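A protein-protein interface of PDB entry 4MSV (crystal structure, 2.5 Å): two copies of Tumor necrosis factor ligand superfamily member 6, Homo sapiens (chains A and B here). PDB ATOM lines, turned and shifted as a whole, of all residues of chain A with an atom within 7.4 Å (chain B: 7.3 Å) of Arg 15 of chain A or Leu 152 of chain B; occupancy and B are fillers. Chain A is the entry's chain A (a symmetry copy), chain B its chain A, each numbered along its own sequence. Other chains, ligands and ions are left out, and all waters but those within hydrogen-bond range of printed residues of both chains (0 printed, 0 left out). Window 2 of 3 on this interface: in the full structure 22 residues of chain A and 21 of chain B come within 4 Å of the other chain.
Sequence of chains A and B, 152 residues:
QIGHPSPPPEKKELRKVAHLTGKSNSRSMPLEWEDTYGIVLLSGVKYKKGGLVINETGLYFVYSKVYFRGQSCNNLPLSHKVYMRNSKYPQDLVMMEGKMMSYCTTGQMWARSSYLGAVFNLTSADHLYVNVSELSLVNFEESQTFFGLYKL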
ATOM      1  N   LEU A  14      21.933  -2.745 -18.610  1.00  0.00           N
ATOM      2  CA  LEU A  14      21.888  -3.338 -20.004  1.00  0.00           C
ATOM      3  C   LEU A  14      22.568  -2.480 -21.090  1.00  0.00           C
ATOM      4  O   LEU A  14      22.226  -1.297 -21.294  1.00  0.00           O
ATOM      5  CB  LEU A  14      20.457  -3.732 -20.470  1.00  0.00           C
ATOM      6  CG  LEU A  14      20.074  -5.252 -20.441  1.00  0.00           C
ATOM      7  CD1 LEU A  14      18.990  -5.585 -21.485  1.00  0.00           C
ATOM      8  CD2 LEU A  14      21.237  -6.251 -20.603  1.00  0.00           C
ATOM      9  N   ARG A  15      23.495  -3.145 -21.794  1.00  0.00           N
ATOM     10  CA  ARG A  15      24.404  -2.549 -22.789  1.00  0.00           C
ATOM     11  C   ARG A  15      23.698  -1.943 -24.015  1.00  0.00           C
ATOM     12  O   ARG A  15      22.843  -2.575 -24.630  1.00  0.00           O
ATOM     13  CB  ARG A  15      25.423  -3.593 -23.225  1.00  0.00           C
ATOM     14  CG  ARG A  15      26.664  -2.979 -23.811  1.00  0.00           C
ATOM     15  CD  ARG A  15      27.900  -3.597 -23.196  1.00  0.00           C
ATOM     16  NE  ARG A  15      29.010  -2.653 -23.337  1.00  0.00           N
ATOM     17  CZ  ARG A  15      30.165  -2.719 -22.679  1.00  0.00           C
ATOM     18  NH1 ARG A  15      30.397  -3.695 -21.801  1.00  0.00           N
ATOM     19  NH2 ARG A  15      31.101  -1.797 -22.917  1.00  0.00           N
ATOM     20  N   LYS A  16      24.015  -0.694 -24.338  1.00  0.00           N
ATOM     21  CA  LYS A  16      23.450  -0.120 -25.528  1.00  0.00           C
ATOM     22  C   LYS A  16      24.147  -0.757 -26.737  1.00  0.00           C
ATOM     23  O   LYS A  16      25.387  -0.778 -26.817  1.00  0.00           O
ATOM     24  CB  LYS A  16      23.626   1.378 -25.616  1.00  0.00           C
ATOM     25  CG  LYS A  16      23.430   2.156 -24.354  1.00  0.00           C
ATOM     26  CD  LYS A  16      22.012   2.193 -23.916  1.00  0.00           C
ATOM     27  CE  LYS A  16      21.956   2.641 -22.459  1.00  0.00           C
ATOM     28  NZ  LYS A  16      21.122   3.868 -22.364  1.00  0.00           N
ATOM     29  N   VAL A  17      23.360  -1.275 -27.673  1.00  0.00           N
ATOM     30  CA  VAL A  17      23.946  -2.064 -28.746  1.00  0.00           C
ATOM     31  C   VAL A  17      22.999  -2.174 -29.896  1.00  0.00           C
ATOM     32  O   VAL A  17      21.769  -2.085 -29.738  1.00  0.00           O
ATOM     33  CB  VAL A  17      24.357  -3.454 -28.229  1.00  0.00           C
ATOM     34  CG1 VAL A  17      23.154  -4.339 -27.964  1.00  0.00           C
ATOM     35  CG2 VAL A  17      25.241  -4.150 -29.194  1.00  0.00           C
ATOM     36  N   ALA A  18      23.576  -2.271 -31.070  1.00  0.00           N
ATOM     37  CA  ALA A  18      22.801  -2.510 -32.275  1.00  0.00           C
ATOM     38  C   ALA A  18      23.626  -3.287 -33.250  1.00  0.00           C
ATOM     39  O   ALA A  18      24.791  -2.996 -33.417  1.00  0.00           O
ATOM     40  CB  ALA A  18      22.352  -1.227 -32.913  1.00  0.00           C
ATOM     41  N   LEU A  41      20.426  -7.329 -33.237  1.00  0.00           N
ATOM     42  CA  LEU A  41      20.364  -6.797 -31.870  1.00  0.00           C
ATOM     43  C   LEU A  41      19.974  -5.318 -31.940  1.00  0.00           C
ATOM     44  O   LEU A  41      20.375  -4.568 -32.851  1.00  0.00           O
ATOM     45  CB  LEU A  41      21.730  -6.821 -31.214  1.00  0.00           C
ATOM     46  CG  LEU A  41      22.400  -8.162 -31.134  1.00  0.00           C
ATOM     47  CD1 LEU A  41      23.841  -8.016 -30.658  1.00  0.00           C
ATOM     48  CD2 LEU A  41      21.589  -8.961 -30.108  1.00  0.00           C
ATOM     49  N   LEU A  42      19.227  -4.899 -30.944  1.00  0.00           N
ATOM     50  CA  LEU A  42      18.839  -3.532 -30.793  1.00  0.00           C
ATOM     51  C   LEU A  42      18.380  -3.345 -29.350  1.00  0.00           C
ATOM     52  O   LEU A  42      17.359  -3.811 -28.956  1.00  0.00           O
ATOM     53  CB  LEU A  42      17.732  -3.205 -31.758  1.00  0.00           C
ATOM     54  CG  LEU A  42      17.390  -1.753 -31.813  1.00  0.00           C
ATOM     55  CD1 LEU A  42      18.565  -0.976 -32.457  1.00  0.00           C
ATOM     56  CD2 LEU A  42      16.044  -1.515 -32.535  1.00  0.00           C
ATOM     57  N   SER A  43      19.165  -2.638 -28.573  1.00  0.00           N
ATOM     58  CA  SER A  43      18.892  -2.449 -27.192  1.00  0.00           C
ATOM     59  C   SER A  43      19.459  -1.107 -26.727  1.00  0.00           C
ATOM     60  O   SER A  43      20.659  -0.849 -26.847  1.00  0.00           O
ATOM     61  CB  SER A  43      19.538  -3.589 -26.470  1.00  0.00           C
ATOM     62  OG  SER A  43      19.400  -3.367 -25.103  1.00  0.00           O
ATOM     63  N   GLY A  44      18.571  -0.259 -26.225  1.00  0.00           N
ATOM     64  CA  GLY A  44      18.899   1.109 -25.752  1.00  0.00           C
ATOM     65  C   GLY A  44      19.372   2.038 -26.871  1.00  0.00           C
ATOM     66  O   GLY A  44      20.232   2.872 -26.680  1.00  0.00           O
ATOM     67  N   VAL A  45      18.812   1.869 -28.047  1.00  0.00           N
ATOM     68  CA  VAL A  45      19.193   2.579 -29.206  1.00  0.00           C
ATOM     69  C   VAL A  45      17.970   2.254 -30.023  1.00  0.00           C
ATOM     70  O   VAL A  45      17.453   1.148 -29.901  1.00  0.00           O
ATOM     71  CB  VAL A  45      20.411   1.912 -29.855  1.00  0.00           C
ATOM     72  CG1 VAL A  45      20.507   2.263 -31.304  1.00  0.00           C
ATOM     73  CG2 VAL A  45      21.695   2.361 -29.208  1.00  0.00           C
ATOM     74  N   LEU A 149      26.548  -0.854 -33.772  1.00  0.00           N
ATOM     75  CA  LEU A 149      27.339  -0.062 -32.846  1.00  0.00           C
ATOM     76  C   LEU A 149      27.214  -0.561 -31.462  1.00  0.00           C
ATOM     77  O   LEU A 149      26.318  -1.373 -31.153  1.00  0.00           O
ATOM     78  CB  LEU A 149      26.965   1.405 -32.844  1.00  0.00           C
ATOM     79  CG  LEU A 149      25.471   1.769 -32.767  1.00  0.00           C
ATOM     80  CD1 LEU A 149      24.960   1.686 -31.371  1.00  0.00           C
ATOM     81  CD2 LEU A 149      25.216   3.152 -33.263  1.00  0.00           C
ATOM     82  N   TYR A 150      28.146  -0.109 -30.618  1.00  0.00           N
ATOM     83  CA  TYR A 150      27.977  -0.342 -29.197  1.00  0.00           C
ATOM     84  C   TYR A 150      28.606   0.729 -28.355  1.00  0.00           C
ATOM     85  O   TYR A 150      29.558   1.344 -28.739  1.00  0.00           O
ATOM     86  CB  TYR A 150      28.425  -1.748 -28.753  1.00  0.00           C
ATOM     87  CG  TYR A 150      29.855  -2.043 -28.934  1.00  0.00           C
ATOM     88  CD1 TYR A 150      30.305  -2.527 -30.135  1.00  0.00           C
ATOM     89  CD2 TYR A 150      30.773  -1.784 -27.940  1.00  0.00           C
ATOM     90  CE1 TYR A 150      31.645  -2.722 -30.358  1.00  0.00           C
ATOM     91  CE2 TYR A 150      32.142  -1.984 -28.166  1.00  0.00           C
ATOM     92  CZ  TYR A 150      32.537  -2.471 -29.372  1.00  0.00           C
ATOM     93  OH  TYR A 150      33.835  -2.741 -29.654  1.00  0.00           O
ATOM     94  N   LYS A 151      28.020   0.944 -27.195  1.00  0.00           N
ATOM     95  CA  LYS A 151      28.517   1.921 -26.276  1.00  0.00           C
ATOM     96  C   LYS A 151      29.724   1.389 -25.554  1.00  0.00           C
ATOM     97  O   LYS A 151      29.658   0.339 -24.997  1.00  0.00           O
ATOM     98  CB  LYS A 151      27.444   2.248 -25.251  1.00  0.00           C
ATOM     99  CG  LYS A 151      27.848   3.423 -24.393  1.00  0.00           C
ATOM    100  CD  LYS A 151      26.679   4.077 -23.716  1.00  0.00           C
ATOM    101  CE  LYS A 151      27.045   5.508 -23.405  1.00  0.00           C
ATOM    102  NZ  LYS A 151      28.253   5.545 -22.535  1.00  0.00           N
ATOM    103  N   LEU A 152      30.823   2.111 -25.541  1.00  0.00           N
ATOM    104  CA  LEU A 152      31.978   1.577 -24.851  1.00  0.00           C
ATOM    105  C   LEU A 152      31.811   1.458 -23.315  1.00  0.00           C
ATOM    106  O   LEU A 152      31.254   2.378 -22.664  1.00  0.00           O
ATOM    107  CB  LEU A 152      33.184   2.434 -25.205  1.00  0.00           C
ATOM    108  CG  LEU A 152      33.545   2.337 -26.681  1.00  0.00           C
ATOM    109  CD1 LEU A 152      34.830   3.083 -26.895  1.00  0.00           C
ATOM    110  CD2 LEU A 152      33.722   0.888 -27.059  1.00  0.00           C
ATOM    111  N   ARG B  15      38.975 -10.302 -18.216  1.00  0.00           N
ATOM    112  CA  ARG B  15      38.257 -10.125 -19.490  1.00  0.00           C
ATOM    113  C   ARG B  15      38.300 -11.349 -20.421  1.00  0.00           C
ATOM    114  O   ARG B  15      39.360 -11.918 -20.672  1.00  0.00           O
ATOM    115  CB  ARG B  15      38.801  -8.895 -20.205  1.00  0.00           C
ATOM    116  CG  ARG B  15      37.835  -8.337 -21.213  1.00  0.00           C
ATOM    117  CD  ARG B  15      37.694  -6.842 -21.037  1.00  0.00           C
ATOM    118  NE  ARG B  15      36.406  -6.429 -21.598  1.00  0.00           N
ATOM    119  CZ  ARG B  15      35.811  -5.259 -21.380  1.00  0.00           C
ATOM    120  NH1 ARG B  15      36.374  -4.342 -20.593  1.00  0.00           N
ATOM    121  NH2 ARG B  15      34.640  -5.006 -21.970  1.00  0.00           N
ATOM    122  N   LYS B  16      37.139 -11.791 -20.892  1.00  0.00           N
ATOM    123  CA  LYS B  16      37.139 -12.874 -21.837  1.00  0.00           C
ATOM    124  C   LYS B  16      37.633 -12.327 -23.182  1.00  0.00           C
ATOM    125  O   LYS B  16      37.115 -11.316 -23.686  1.00  0.00           O
ATOM    126  CB  LYS B  16      35.775 -13.487 -22.049  1.00  0.00           C
ATOM    127  CG  LYS B  16      34.923 -13.675 -20.834  1.00  0.00           C
ATOM    128  CD  LYS B  16      35.433 -14.740 -19.933  1.00  0.00           C
ATOM    129  CE  LYS B  16      34.764 -14.595 -18.570  1.00  0.00           C
ATOM    130  NZ  LYS B  16      34.049 -15.858 -18.248  1.00  0.00           N
ATOM    131  N   GLY B  58      26.612 -14.154 -23.615  1.00  0.00           N
ATOM    132  CA  GLY B  58      26.580 -12.685 -23.675  1.00  0.00           C
ATOM    133  C   GLY B  58      26.954 -12.074 -25.004  1.00  0.00           C
ATOM    134  O   GLY B  58      27.031 -12.772 -26.027  1.00  0.00           O
ATOM    135  N   LEU B  59      27.205 -10.768 -24.969  1.00  0.00           N
ATOM    136  CA  LEU B  59      27.616 -10.009 -26.165  1.00  0.00           C
ATOM    137  C   LEU B  59      29.119  -9.982 -26.395  1.00  0.00           C
ATOM    138  O   LEU B  59      29.916  -9.584 -25.522  1.00  0.00           O
ATOM    139  CB  LEU B  59      27.151  -8.553 -26.029  1.00  0.00           C
ATOM    140  CG  LEU B  59      25.620  -8.383 -25.971  1.00  0.00           C
ATOM    141  CD1 LEU B  59      25.225  -6.954 -25.757  1.00  0.00           C
ATOM    142  CD2 LEU B  59      24.971  -8.841 -27.222  1.00  0.00           C
ATOM    143  N   TYR B  60      29.498 -10.361 -27.601  1.00  0.00           N
ATOM    144  CA  TYR B  60      30.910 -10.335 -27.975  1.00  0.00           C
ATOM    145  C   TYR B  60      31.083  -9.653 -29.309  1.00  0.00           C
ATOM    146  O   TYR B  60      30.260  -9.819 -30.225  1.00  0.00           O
ATOM    147  CB  TYR B  60      31.497 -11.746 -28.120  1.00  0.00           C
ATOM    148  CG  TYR B  60      31.541 -12.597 -26.892  1.00  0.00           C
ATOM    149  CD1 TYR B  60      30.399 -13.146 -26.360  1.00  0.00           C
ATOM    150  CD2 TYR B  60      32.737 -12.884 -26.283  1.00  0.00           C
ATOM    151  CE1 TYR B  60      30.438 -13.969 -25.264  1.00  0.00           C
ATOM    152  CE2 TYR B  60      32.795 -13.710 -25.164  1.00  0.00           C
ATOM    153  CZ  TYR B  60      31.647 -14.252 -24.676  1.00  0.00           C
ATOM    154  OH  TYR B  60      31.715 -15.049 -23.584  1.00  0.00           O
ATOM    155  N   PHE B  61      32.177  -8.942 -29.448  1.00  0.00           N
ATOM    156  CA  PHE B  61      32.577  -8.444 -30.757  1.00  0.00           C
ATOM    157  C   PHE B  61      33.525  -9.474 -31.306  1.00  0.00           C
ATOM    158  O   PHE B  61      34.463  -9.841 -30.623  1.00  0.00           O
ATOM    159  CB  PHE B  61      33.312  -7.121 -30.601  1.00  0.00           C
ATOM    160  CG  PHE B  61      33.721  -6.529 -31.895  1.00  0.00           C
ATOM    161  CD1 PHE B  61      32.847  -5.809 -32.644  1.00  0.00           C
ATOM    162  CD2 PHE B  61      35.002  -6.635 -32.333  1.00  0.00           C
ATOM    163  CE1 PHE B  61      33.218  -5.243 -33.851  1.00  0.00           C
ATOM    164  CE2 PHE B  61      35.391  -6.066 -33.513  1.00  0.00           C
ATOM    165  CZ  PHE B  61      34.484  -5.409 -34.294  1.00  0.00           C
ATOM    166  N   VAL B 119      29.282  -7.262 -33.786  1.00  0.00           N
ATOM    167  CA  VAL B 119      28.793  -7.728 -32.492  1.00  0.00           C
ATOM    168  C   VAL B 119      27.754  -8.868 -32.595  1.00  0.00           C
ATOM    169  O   VAL B 119      26.871  -8.845 -33.428  1.00  0.00           O
ATOM    170  CB  VAL B 119      28.117  -6.590 -31.732  1.00  0.00           C
ATOM    171  CG1 VAL B 119      27.738  -7.072 -30.354  1.00  0.00           C
ATOM    172  CG2 VAL B 119      29.062  -5.440 -31.590  1.00  0.00           C
ATOM    173  N   PHE B 120      27.854  -9.836 -31.701  1.00  0.00           N
ATOM    174  CA  PHE B 120      26.896 -10.926 -31.660  1.00  0.00           C
ATOM    175  C   PHE B 120      26.638 -11.339 -30.248  1.00  0.00           C
ATOM    176  O   PHE B 120      27.524 -11.249 -29.364  1.00  0.00           O
ATOM    177  CB  PHE B 120      27.359 -12.151 -32.441  1.00  0.00           C
ATOM    178  CG  PHE B 120      27.657 -11.849 -33.837  1.00  0.00           C
ATOM    179  CD1 PHE B 120      28.914 -11.416 -34.219  1.00  0.00           C
ATOM    180  CD2 PHE B 120      26.694 -11.944 -34.764  1.00  0.00           C
ATOM    181  CE1 PHE B 120      29.236 -11.137 -35.561  1.00  0.00           C
ATOM    182  CE2 PHE B 120      26.972 -11.663 -36.080  1.00  0.00           C
ATOM    183  CZ  PHE B 120      28.259 -11.247 -36.488  1.00  0.00           C
ATOM    184  N   TYR B 150      36.093 -10.440 -28.235  1.00  0.00           N
ATOM    185  CA  TYR B 150      36.074 -10.064 -26.834  1.00  0.00           C
ATOM    186  C   TYR B 150      34.686  -9.834 -26.313  1.00  0.00           C
ATOM    187  O   TYR B 150      33.807  -9.458 -27.032  1.00  0.00           O
ATOM    188  CB  TYR B 150      37.007  -8.881 -26.509  1.00  0.00           C
ATOM    189  CG  TYR B 150      36.663  -7.608 -27.162  1.00  0.00           C
ATOM    190  CD1 TYR B 150      37.133  -7.338 -28.421  1.00  0.00           C
ATOM    191  CD2 TYR B 150      35.820  -6.697 -26.562  1.00  0.00           C
ATOM    192  CE1 TYR B 150      36.751  -6.199 -29.086  1.00  0.00           C
ATOM    193  CE2 TYR B 150      35.430  -5.534 -27.240  1.00  0.00           C
ATOM    194  CZ  TYR B 150      35.929  -5.308 -28.484  1.00  0.00           C
ATOM    195  OH  TYR B 150      35.643  -4.185 -29.186  1.00  0.00           O
ATOM    196  N   LYS B 151      34.520 -10.095 -25.033  1.00  0.00           N
ATOM    197  CA  LYS B 151      33.257  -9.906 -24.390  1.00  0.00           C
ATOM    198  C   LYS B 151      33.031  -8.446 -24.108  1.00  0.00           C
ATOM    199  O   LYS B 151      33.858  -7.829 -23.515  1.00  0.00           O
ATOM    200  CB  LYS B 151      33.238 -10.663 -23.072  1.00  0.00           C
ATOM    201  CG  LYS B 151      31.856 -10.664 -22.463  1.00  0.00           C
ATOM    202  CD  LYS B 151      31.668 -11.757 -21.453  1.00  0.00           C
ATOM    203  CE  LYS B 151      30.195 -12.070 -21.354  1.00  0.00           C
ATOM    204  NZ  LYS B 151      29.442 -10.847 -20.961  1.00  0.00           N
ATOM    205  N   LEU B 152      31.909  -7.890 -24.510  1.00  0.00           N
ATOM    206  CA  LEU B 152      31.715  -6.482 -24.241  1.00  0.00           C
ATOM    207  C   LEU B 152      31.573  -6.128 -22.738  1.00  0.00           C
ATOM    208  O   LEU B 152      30.885  -6.855 -21.978  1.00  0.00           O
ATOM    209  CB  LEU B 152      30.503  -6.007 -25.030  1.00  0.00           C
ATOM    210  CG  LEU B 152      30.735  -6.077 -26.534  1.00  0.00           C
ATOM    211  CD1 LEU B 152      29.556  -5.444 -27.214  1.00  0.00           C
ATOM    212  CD2 LEU B 152      31.995  -5.327 -26.882  1.00  0.00           C
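Arg 15 of chain A touches Leu 152 of chain B, but with the chains exchanged Leu 152 of chain A does not touch Arg 15 of chain B (7.2 Å).
Tyr 150 of chain A touches its own counterpart, Tyr 150 of chain B.
Tyr 150 of chain A touches Leu 152 of chain B, but with the chains exchanged Leu 152 of chain A does not touch Tyr 150 of chain B (5.8 Å).
Positions printed for both chains: 15, 16, 150, 151 and 152.
Hydrophobic or aromatic side chains of chain A within 4 Å of the printed part of chain B: Val 17, Leu 41 and Tyr 150.
Along chain A the printed residues that touch a printed residue of chain B span positions 15 to 150.
Of the 11 printed residues of chain B, 4 touch a printed residue of chain A.
Hydrophobic or aromatic side chains of chain B within 4 Å of the printed part of chain A: Leu 59, Val 119, Tyr 150 and Leu 152.
Among the printed residues, no Asp or Glu carboxylate lies within 4 Å of a Lys or Arg side-chain nitrogen of the other chain.
O of Leu 59 of chain B sits at hydrogen-bond distance from N of Leu 152 of chain B (2.8 Å).
The backbone NH (N) of Tyr 150 of chain B sits at hydrogen-bond distance from the backbone carbonyl oxygen (O) of Phe 61 of chain B, 3.0 Å away.
The guanidinium group of Arg 15 of chain A is in hydrogen-bond range of the backbone carbonyl oxygen of Lys 151 of chain A (3.3 Å).
N of Val 17 of chain A sits at hydrogen-bond distance from O of Ser 43 of chain A (2.9 Å).
Leu 152 of chain B touches just these residues of chain A: Arg 15 (2.9 Å) and Tyr 150 (3.6 Å).
Of the printed residues of chain B, Tyr 150 of chain A touches Val 119 (3.5 Å), Tyr 150 (2.4 Å) and Leu 152 (3.6 Å).
Printed residues of chain A within 4 Å of Val 119 of chain B: Tyr 150 (3.5 Å).
Phe 120 of chain B touches none of the printed residues of chain A.
Lys 16 of chain B touches none of the printed residues of chain A.
The nearest residue of chain A that does not touch Leu 152 of chain B is Val 17 of chain A (4.9 Å).
Leu 59 of chain B touches Val 17 of chain A.
Leu 59 of chain B touches Leu 41 of chain A.
Tyr 150 of chain A touches Val 119 of chain B.
Tyr 150 of chain A touches Leu 152 of chain B.
O of Leu 152 of chain B sits close to NH1 of Arg 15 of chain A.
The side-chain hydroxyl (OH) of Tyr 150 of chain A sits close to the side-chain hydroxyl (OH) of Tyr 150 of chain B (2.4 Å).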
